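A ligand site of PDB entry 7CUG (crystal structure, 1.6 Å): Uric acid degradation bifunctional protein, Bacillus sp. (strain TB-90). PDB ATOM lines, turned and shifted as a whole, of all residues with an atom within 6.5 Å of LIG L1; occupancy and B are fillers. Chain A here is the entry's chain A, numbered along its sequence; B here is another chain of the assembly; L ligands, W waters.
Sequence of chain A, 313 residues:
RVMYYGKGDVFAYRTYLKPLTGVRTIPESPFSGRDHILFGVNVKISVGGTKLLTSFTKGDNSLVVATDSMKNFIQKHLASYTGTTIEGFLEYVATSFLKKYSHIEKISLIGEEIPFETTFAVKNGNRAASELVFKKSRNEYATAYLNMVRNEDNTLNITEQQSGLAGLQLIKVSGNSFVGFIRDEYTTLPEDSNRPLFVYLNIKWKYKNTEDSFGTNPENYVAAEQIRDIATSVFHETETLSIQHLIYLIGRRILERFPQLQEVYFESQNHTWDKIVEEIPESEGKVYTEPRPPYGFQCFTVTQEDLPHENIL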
ATOM      1  N   SER A 177     -17.030 -26.897 -29.777  1.00  0.00           N
ATOM      2  CA  SER A 177     -17.035 -25.699 -28.966  1.00  0.00           C
ATOM      3  C   SER A 177     -16.441 -25.984 -27.583  1.00  0.00           C
ATOM      4  O   SER A 177     -16.355 -27.137 -27.141  1.00  0.00           O
ATOM      5  CB  SER A 177     -18.442 -25.112 -28.786  1.00  0.00           C
ATOM      6  OG  SER A 177     -19.264 -25.944 -28.004  1.00  0.00           O
ATOM      7  N   PHE A 178     -16.037 -24.899 -26.924  1.00  0.00           N
ATOM      8  CA  PHE A 178     -15.656 -24.922 -25.512  1.00  0.00           C
ATOM      9  C   PHE A 178     -16.057 -23.562 -24.952  1.00  0.00           C
ATOM     10  O   PHE A 178     -15.328 -22.567 -25.115  1.00  0.00           O
ATOM     11  CB  PHE A 178     -14.172 -25.194 -25.324  1.00  0.00           C
ATOM     12  CG  PHE A 178     -13.814 -25.429 -23.882  1.00  0.00           C
ATOM     13  CD1 PHE A 178     -14.462 -26.430 -23.145  1.00  0.00           C
ATOM     14  CD2 PHE A 178     -12.855 -24.650 -23.272  1.00  0.00           C
ATOM     15  CE1 PHE A 178     -14.148 -26.630 -21.795  1.00  0.00           C
ATOM     16  CE2 PHE A 178     -12.537 -24.842 -21.944  1.00  0.00           C
ATOM     17  CZ  PHE A 178     -13.173 -25.857 -21.184  1.00  0.00           C
ATOM     18  N   PHE A 181     -17.245 -22.105 -19.430  1.00  0.00           N
ATOM     19  CA  PHE A 181     -16.373 -22.511 -18.347  1.00  0.00           C
ATOM     20  C   PHE A 181     -16.100 -21.311 -17.418  1.00  0.00           C
ATOM     21  O   PHE A 181     -16.439 -20.161 -17.713  1.00  0.00           O
ATOM     22  CB  PHE A 181     -15.087 -23.122 -18.907  1.00  0.00           C
ATOM     23  CG  PHE A 181     -14.348 -22.236 -19.855  1.00  0.00           C
ATOM     24  CD1 PHE A 181     -13.477 -21.245 -19.402  1.00  0.00           C
ATOM     25  CD2 PHE A 181     -14.489 -22.411 -21.215  1.00  0.00           C
ATOM     26  CE1 PHE A 181     -12.731 -20.484 -20.286  1.00  0.00           C
ATOM     27  CE2 PHE A 181     -13.806 -21.557 -22.135  1.00  0.00           C
ATOM     28  CZ  PHE A 181     -12.892 -20.609 -21.633  1.00  0.00           C
ATOM     29  N   LEU A 189      -8.334 -17.894 -21.007  1.00  0.00           N
ATOM     30  CA  LEU A 189      -8.718 -18.633 -22.200  1.00  0.00           C
ATOM     31  C   LEU A 189      -9.996 -18.048 -22.798  1.00  0.00           C
ATOM     32  O   LEU A 189     -11.043 -18.037 -22.137  1.00  0.00           O
ATOM     33  CB  LEU A 189      -8.915 -20.122 -21.853  1.00  0.00           C
ATOM     34  CG  LEU A 189      -9.314 -21.038 -23.008  1.00  0.00           C
ATOM     35  CD1 LEU A 189      -8.215 -21.089 -24.057  1.00  0.00           C
ATOM     36  CD2 LEU A 189      -9.690 -22.458 -22.519  1.00  0.00           C
ATOM     37  N   ARG A 195     -13.795 -24.643 -32.689  1.00  0.00           N
ATOM     38  CA  ARG A 195     -12.364 -24.855 -32.625  1.00  0.00           C
ATOM     39  C   ARG A 195     -11.989 -26.167 -33.286  1.00  0.00           C
ATOM     40  O   ARG A 195     -12.808 -27.093 -33.321  1.00  0.00           O
ATOM     41  CB  ARG A 195     -11.888 -24.898 -31.168  1.00  0.00           C
ATOM     42  CG  ARG A 195     -12.525 -25.993 -30.322  1.00  0.00           C
ATOM     43  CD  ARG A 195     -11.868 -26.112 -28.991  1.00  0.00           C
ATOM     44  NE  ARG A 195     -12.490 -27.133 -28.165  1.00  0.00           N
ATOM     45  CZ  ARG A 195     -12.050 -27.547 -26.988  1.00  0.00           C
ATOM     46  NH1 ARG A 195     -10.942 -27.015 -26.466  1.00  0.00           N
ATOM     47  NH2 ARG A 195     -12.703 -28.488 -26.319  1.00  0.00           N
ATOM     48  N   LEU A 197     -10.659 -29.139 -32.648  1.00  0.00           N
ATOM     49  CA  LEU A 197     -10.280 -29.932 -31.490  1.00  0.00           C
ATOM     50  C   LEU A 197      -9.339 -31.053 -31.892  1.00  0.00           C
ATOM     51  O   LEU A 197      -9.650 -31.874 -32.757  1.00  0.00           O
ATOM     52  CB  LEU A 197     -11.524 -30.498 -30.812  1.00  0.00           C
ATOM     53  CG  LEU A 197     -11.310 -31.398 -29.583  1.00  0.00           C
ATOM     54  CD1 LEU A 197     -10.454 -30.680 -28.544  1.00  0.00           C
ATOM     55  CD2 LEU A 197     -12.666 -31.726 -28.987  1.00  0.00           C
ATOM     56  N   LEU A 241     -18.791 -30.397 -27.009  1.00  0.00           N
ATOM     57  CA  LEU A 241     -18.895 -29.269 -26.077  1.00  0.00           C
ATOM     58  C   LEU A 241     -17.667 -29.159 -25.197  1.00  0.00           C
ATOM     59  O   LEU A 241     -17.570 -28.166 -24.459  1.00  0.00           O
ATOM     60  CB  LEU A 241     -20.140 -29.420 -25.176  1.00  0.00           C
ATOM     61  CG  LEU A 241     -21.479 -29.416 -25.945  1.00  0.00           C
ATOM     62  CD1 LEU A 241     -22.602 -29.946 -25.060  1.00  0.00           C
ATOM     63  CD2 LEU A 241     -21.845 -28.028 -26.460  1.00  0.00           C
ATOM     64  N   SER A 242     -16.754 -30.181 -25.278  1.00  0.00           N
ATOM     65  CA  SER A 242     -15.526 -30.321 -24.513  1.00  0.00           C
ATOM     66  C   SER A 242     -15.030 -31.728 -24.815  1.00  0.00           C
ATOM     67  O   SER A 242     -15.789 -32.555 -25.355  1.00  0.00           O
ATOM     68  CB  SER A 242     -15.720 -30.206 -23.015  1.00  0.00           C
ATOM     69  OG  SER A 242     -16.556 -31.220 -22.546  1.00  0.00           O
ATOM     70  N   ILE A 243     -13.744 -31.973 -24.520  1.00  0.00           N
ATOM     71  CA  ILE A 243     -13.259 -33.350 -24.626  1.00  0.00           C
ATOM     72  C   ILE A 243     -14.014 -34.281 -23.670  1.00  0.00           C
ATOM     73  O   ILE A 243     -14.326 -35.442 -23.995  1.00  0.00           O
ATOM     74  CB  ILE A 243     -11.748 -33.405 -24.383  1.00  0.00           C
ATOM     75  CG1 ILE A 243     -11.025 -32.669 -25.505  1.00  0.00           C
ATOM     76  CG2 ILE A 243     -11.297 -34.885 -24.298  1.00  0.00           C
ATOM     77  CD1 ILE A 243      -9.535 -32.429 -25.162  1.00  0.00           C
ATOM     78  N   GLN A 244     -14.301 -33.778 -22.468  1.00  0.00           N
ATOM     79  CA  GLN A 244     -15.079 -34.533 -21.492  1.00  0.00           C
ATOM     80  C   GLN A 244     -16.373 -35.047 -22.100  1.00  0.00           C
ATOM     81  O   GLN A 244     -16.676 -36.238 -22.053  1.00  0.00           O
ATOM     82  CB  GLN A 244     -15.357 -33.648 -20.277  1.00  0.00           C
ATOM     83  CG  GLN A 244     -14.163 -33.321 -19.370  1.00  0.00           C
ATOM     84  CD  GLN A 244     -13.388 -32.057 -19.752  1.00  0.00           C
ATOM     85  OE1 GLN A 244     -13.086 -31.813 -20.919  1.00  0.00           O
ATOM     86  NE2 GLN A 244     -13.034 -31.251 -18.742  1.00  0.00           N
ATOM     87  N   ASN A 270      -5.549 -32.883 -24.680  1.00  0.00           N
ATOM     88  CA  ASN A 270      -5.930 -31.807 -25.586  1.00  0.00           C
ATOM     89  C   ASN A 270      -4.664 -31.221 -26.189  1.00  0.00           C
ATOM     90  O   ASN A 270      -3.837 -30.688 -25.448  1.00  0.00           O
ATOM     91  CB  ASN A 270      -6.711 -30.711 -24.852  1.00  0.00           C
ATOM     92  CG  ASN A 270      -7.313 -29.690 -25.788  1.00  0.00           C
ATOM     93  OD1 ASN A 270      -6.915 -29.591 -26.974  1.00  0.00           O
ATOM     94  ND2 ASN A 270      -8.243 -28.916 -25.282  1.00  0.00           N
ATOM     95  N   GLY A 296      -3.938 -30.057 -21.672  1.00  0.00           N
ATOM     96  CA  GLY A 296      -5.015 -30.546 -20.809  1.00  0.00           C
ATOM     97  C   GLY A 296      -5.122 -32.064 -20.910  1.00  0.00           C
ATOM     98  O   GLY A 296      -4.832 -32.652 -21.940  1.00  0.00           O
ATOM     99  N   PHE A 297      -5.691 -32.689 -19.881  1.00  0.00           N
ATOM    100  CA  PHE A 297      -5.975 -34.119 -19.973  1.00  0.00           C
ATOM    101  C   PHE A 297      -7.217 -34.442 -19.165  1.00  0.00           C
ATOM    102  O   PHE A 297      -7.565 -33.735 -18.205  1.00  0.00           O
ATOM    103  CB  PHE A 297      -4.770 -34.959 -19.516  1.00  0.00           C
ATOM    104  CG  PHE A 297      -4.410 -34.765 -18.091  1.00  0.00           C
ATOM    105  CD1 PHE A 297      -5.137 -35.409 -17.100  1.00  0.00           C
ATOM    106  CD2 PHE A 297      -3.303 -34.016 -17.715  1.00  0.00           C
ATOM    107  CE1 PHE A 297      -4.766 -35.241 -15.721  1.00  0.00           C
ATOM    108  CE2 PHE A 297      -2.972 -33.847 -16.386  1.00  0.00           C
ATOM    109  CZ  PHE A 297      -3.702 -34.432 -15.419  1.00  0.00           C
ATOM    110  N   GLN A 298      -7.880 -35.517 -19.585  1.00  0.00           N
ATOM    111  CA  GLN A 298      -9.071 -36.042 -18.936  1.00  0.00           C
ATOM    112  C   GLN A 298      -8.970 -37.558 -18.739  1.00  0.00           C
ATOM    113  O   GLN A 298      -8.383 -38.269 -19.551  1.00  0.00           O
ATOM    114  CB  GLN A 298     -10.331 -35.744 -19.772  1.00  0.00           C
ATOM    115  CG  GLN A 298     -10.666 -34.310 -19.943  1.00  0.00           C
ATOM    116  CD  GLN A 298      -9.734 -33.609 -20.934  1.00  0.00           C
ATOM    117  OE1 GLN A 298      -9.146 -34.208 -21.830  1.00  0.00           O
ATOM    118  NE2 GLN A 298      -9.642 -32.297 -20.783  1.00  0.00           N
ATOM    119  N   TYR B   5      -9.527 -34.600 -14.198  1.00  0.00           N
ATOM    120  CA  TYR B   5      -8.904 -33.923 -15.323  1.00  0.00           C
ATOM    121  C   TYR B   5      -7.877 -32.946 -14.770  1.00  0.00           C
ATOM    122  O   TYR B   5      -7.787 -32.727 -13.560  1.00  0.00           O
ATOM    123  CB  TYR B   5      -9.979 -33.234 -16.201  1.00  0.00           C
ATOM    124  CG  TYR B   5     -10.526 -31.908 -15.668  1.00  0.00           C
ATOM    125  CD1 TYR B   5     -11.223 -31.846 -14.469  1.00  0.00           C
ATOM    126  CD2 TYR B   5     -10.333 -30.764 -16.372  1.00  0.00           C
ATOM    127  CE1 TYR B   5     -11.692 -30.666 -13.999  1.00  0.00           C
ATOM    128  CE2 TYR B   5     -10.803 -29.558 -15.928  1.00  0.00           C
ATOM    129  CZ  TYR B   5     -11.463 -29.495 -14.723  1.00  0.00           C
ATOM    130  OH  TYR B   5     -11.919 -28.285 -14.279  1.00  0.00           O
ATOM    131  N   LYS B   7      -3.887 -30.681 -15.995  1.00  0.00           N
ATOM    132  CA  LYS B   7      -2.940 -30.137 -16.944  1.00  0.00           C
ATOM    133  C   LYS B   7      -1.555 -30.751 -16.752  1.00  0.00           C
ATOM    134  O   LYS B   7      -1.099 -30.875 -15.619  1.00  0.00           O
ATOM    135  CB  LYS B   7      -2.845 -28.603 -16.731  1.00  0.00           C
ATOM    136  CG  LYS B   7      -2.153 -27.842 -17.908  1.00  0.00           C
ATOM    137  CD  LYS B   7      -3.154 -27.679 -19.033  1.00  0.00           C
ATOM    138  CE  LYS B   7      -2.694 -26.718 -20.133  1.00  0.00           C
ATOM    139  NZ  LYS B   7      -3.817 -26.585 -21.114  1.00  0.00           N
ATOM    140  N   ASN B  61     -20.236 -27.084 -18.726  1.00  0.00           N
ATOM    141  CA  ASN B  61     -18.954 -26.541 -18.302  1.00  0.00           C
ATOM    142  C   ASN B  61     -19.078 -25.564 -17.170  1.00  0.00           C
ATOM    143  O   ASN B  61     -18.058 -24.986 -16.792  1.00  0.00           O
ATOM    144  CB  ASN B  61     -18.257 -25.887 -19.496  1.00  0.00           C
ATOM    145  CG  ASN B  61     -17.881 -26.942 -20.568  1.00  0.00           C
ATOM    146  OD1 ASN B  61     -17.403 -28.024 -20.223  1.00  0.00           O
ATOM    147  ND2 ASN B  61     -18.082 -26.623 -21.833  1.00  0.00           N
ATOM    148  N   VAL B  64     -16.407 -26.154 -14.592  1.00  0.00           N
ATOM    149  CA  VAL B  64     -15.118 -26.550 -15.132  1.00  0.00           C
ATOM    150  C   VAL B  64     -14.176 -25.357 -15.031  1.00  0.00           C
ATOM    151  O   VAL B  64     -14.366 -24.338 -15.715  1.00  0.00           O
ATOM    152  CB  VAL B  64     -15.224 -27.016 -16.593  1.00  0.00           C
ATOM    153  CG1 VAL B  64     -13.822 -27.239 -17.165  1.00  0.00           C
ATOM    154  CG2 VAL B  64     -16.115 -28.287 -16.681  1.00  0.00           C
ATOM    155  N   VAL B  65     -13.156 -25.521 -14.187  1.00  0.00           N
ATOM    156  CA  VAL B  65     -11.953 -24.716 -14.260  1.00  0.00           C
ATOM    157  C   VAL B  65     -11.218 -25.123 -15.507  1.00  0.00           C
ATOM    158  O   VAL B  65     -10.801 -26.281 -15.643  1.00  0.00           O
ATOM    159  CB  VAL B  65     -11.074 -24.946 -13.021  1.00  0.00           C
ATOM    160  CG1 VAL B  65      -9.850 -24.050 -13.081  1.00  0.00           C
ATOM    161  CG2 VAL B  65     -11.846 -24.689 -11.725  1.00  0.00           C
ATOM    162  N   ALA B  66     -11.081 -24.237 -16.460  1.00  0.00           N
ATOM    163  CA  ALA B  66     -10.316 -24.553 -17.659  1.00  0.00           C
ATOM    164  C   ALA B  66      -8.911 -25.035 -17.275  1.00  0.00           C
ATOM    165  O   ALA B  66      -8.248 -24.531 -16.375  1.00  0.00           O
ATOM    166  CB  ALA B  66     -10.231 -23.367 -18.620  1.00  0.00           C
ATOM    167  N   THR B  67      -8.430 -26.042 -17.991  1.00  0.00           N
ATOM    168  CA  THR B  67      -7.082 -26.492 -17.697  1.00  0.00           C
ATOM    169  C   THR B  67      -6.081 -25.388 -17.970  1.00  0.00           C
ATOM    170  O   THR B  67      -5.066 -25.293 -17.270  1.00  0.00           O
ATOM    171  CB  THR B  67      -6.741 -27.748 -18.533  1.00  0.00           C
ATOM    172  OG1 THR B  67      -6.628 -27.427 -19.932  1.00  0.00           O
ATOM    173  CG2 THR B  67      -7.782 -28.804 -18.347  1.00  0.00           C
ATOM    174  N   ASP B  68      -6.386 -24.501 -18.944  1.00  0.00           N
ATOM    175  CA  ASP B  68      -5.538 -23.343 -19.202  1.00  0.00           C
ATOM    176  C   ASP B  68      -5.417 -22.490 -17.966  1.00  0.00           C
ATOM    177  O   ASP B  68      -4.354 -21.928 -17.686  1.00  0.00           O
ATOM    178  CB  ASP B  68      -6.094 -22.517 -20.370  1.00  0.00           C
ATOM    179  CG  ASP B  68      -5.193 -21.361 -20.728  1.00  0.00           C
ATOM    180  OD1 ASP B  68      -4.175 -21.571 -21.404  1.00  0.00           O
ATOM    181  OD2 ASP B  68      -5.511 -20.211 -20.313  1.00  0.00           O
ATOM    182  N   SER B  69      -6.510 -22.391 -17.205  1.00  0.00           N
ATOM    183  CA  SER B  69      -6.507 -21.593 -15.973  1.00  0.00           C
ATOM    184  C   SER B  69      -5.723 -22.294 -14.873  1.00  0.00           C
ATOM    185  O   SER B  69      -5.118 -21.615 -14.025  1.00  0.00           O
ATOM    186  CB  SER B  69      -7.942 -21.321 -15.494  1.00  0.00           C
ATOM    187  OG  SER B  69      -8.659 -20.761 -16.599  1.00  0.00           O
HETATM  188  N1  LIG L   1     -11.858 -29.399 -21.717  1.00  0.00           N
HETATM  189  C1  LIG L   1     -11.744 -29.121 -23.052  1.00  0.00           C
HETATM  190  O1  LIG L   1     -12.327 -29.766 -23.864  1.00  0.00           O
HETATM  191  N2  LIG L   1     -11.013 -28.037 -23.503  1.00  0.00           N
HETATM  192  C2  LIG L   1     -10.379 -27.283 -22.567  1.00  0.00           C
HETATM  193  C3  LIG L   1     -10.487 -27.581 -21.229  1.00  0.00           C
HETATM  194  C4  LIG L   1     -11.219 -28.671 -20.820  1.00  0.00           C
HETATM  195  O2  LIG L   1     -11.321 -28.956 -19.664  1.00  0.00           O
HETATM  196  N3  LIG L   1      -9.741 -26.667 -20.531  1.00  0.00           N
HETATM  197  N4  LIG L   1      -9.152 -25.851 -21.457  1.00  0.00           N
HETATM  198  N5  LIG L   1      -9.568 -26.228 -22.692  1.00  0.00           N
HETATM  199  O1  LG2 L   2      -7.845 -28.963 -22.044  1.00  0.00           O
HETATM  200  O2  LG2 L   2      -8.593 -29.899 -21.690  1.00  0.00           O
HETATM  201  O   HOH W   1      -8.880 -24.749 -25.084  1.00  0.00           O
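The backbone NH (N) of Ile 243 is in hydrogen-bond range of an oxygen (O1) of LIG L1, at 2.7 Å.
An oxygen (O1) of LIG L1 lies within hydrogen-bond range of the guanidinium group (NH2) of Arg 195 (2.8 Å).
The side-chain amide oxygen (OE1) of Gln 244 sits at hydrogen-bond distance from a nitrogen (N1) of LIG L1 (2.8 Å).
The backbone NH of Thr 67 of chain B is in hydrogen-bond range of a nitrogen (N3) of LIG L1, 2.9 Å away.
A nitrogen (N3) of LIG L1 is in hydrogen-bond range of the side-chain hydroxyl of Thr 67 of chain B, 3.3 Å away.
The side-chain amide nitrogen of Asn 270 sits close to a nitrogen (N2) of LIG L1 (3.4 Å).
The side-chain hydroxyl (OG1) of Thr 67 of chain B lies within hydrogen-bond range of an oxygen (O1) of LG2 L2.
The side-chain amide nitrogen (ND2) of Asn 270 lies within hydrogen-bond range of an oxygen (O1) of LG2 L2, 3.3 Å away.
An oxygen (O2) of LG2 L2 is in hydrogen-bond range of the side-chain amide nitrogen of Gln 298.
A nitrogen (N1) of LIG L1 sits close to an oxygen (O2) of LG2 L2.
N of Gln 244 lies close to OG of Ser 242 (3.4 Å).
OE1 of Gln 244 sits at hydrogen-bond distance from NE2 of Gln 298 (3.5 Å).
OG1 of Thr 67 of chain B lies within hydrogen-bond range of NZ of Lys 7 of chain B (3.2 Å).
The backbone NH of Asn 270 lies within hydrogen-bond range of the backbone carbonyl oxygen of Gly 296 (2.8 Å).
The backbone carbonyl oxygen of Val 65 of chain B sits at hydrogen-bond distance from the side-chain hydroxyl of Tyr 5 of chain B.
Merely in contact with LIG L1: Phe 178 (3.2 Å), Ser 242 (3.3 Å), Leu 189 (3.6 Å), Ala 66 of chain B (3.6 Å), Gln 298 (3.8 Å), Tyr 5 of chain B (3.8 Å), Val 64 of chain B (3.9 Å) and Asp 68 of chain B (3.97 Å).
13 residues have an atom within 4 Å of LIG L1: Phe 178, Leu 189, Arg 195, Ser 242, Ile 243, Gln 244, Asn 270, Gln 298, Tyr 5 of chain B, Val 64 of chain B, Ala 66 of chain B, Thr 67 of chain B and Asp 68 of chain B.
The nearest printed residue that does not touch LIG L1 is Val 65 of chain B (4.9 Å).
Water W1 lies within hydrogen-bond range of N5 of LIG L1 and NH1 of Arg 195.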
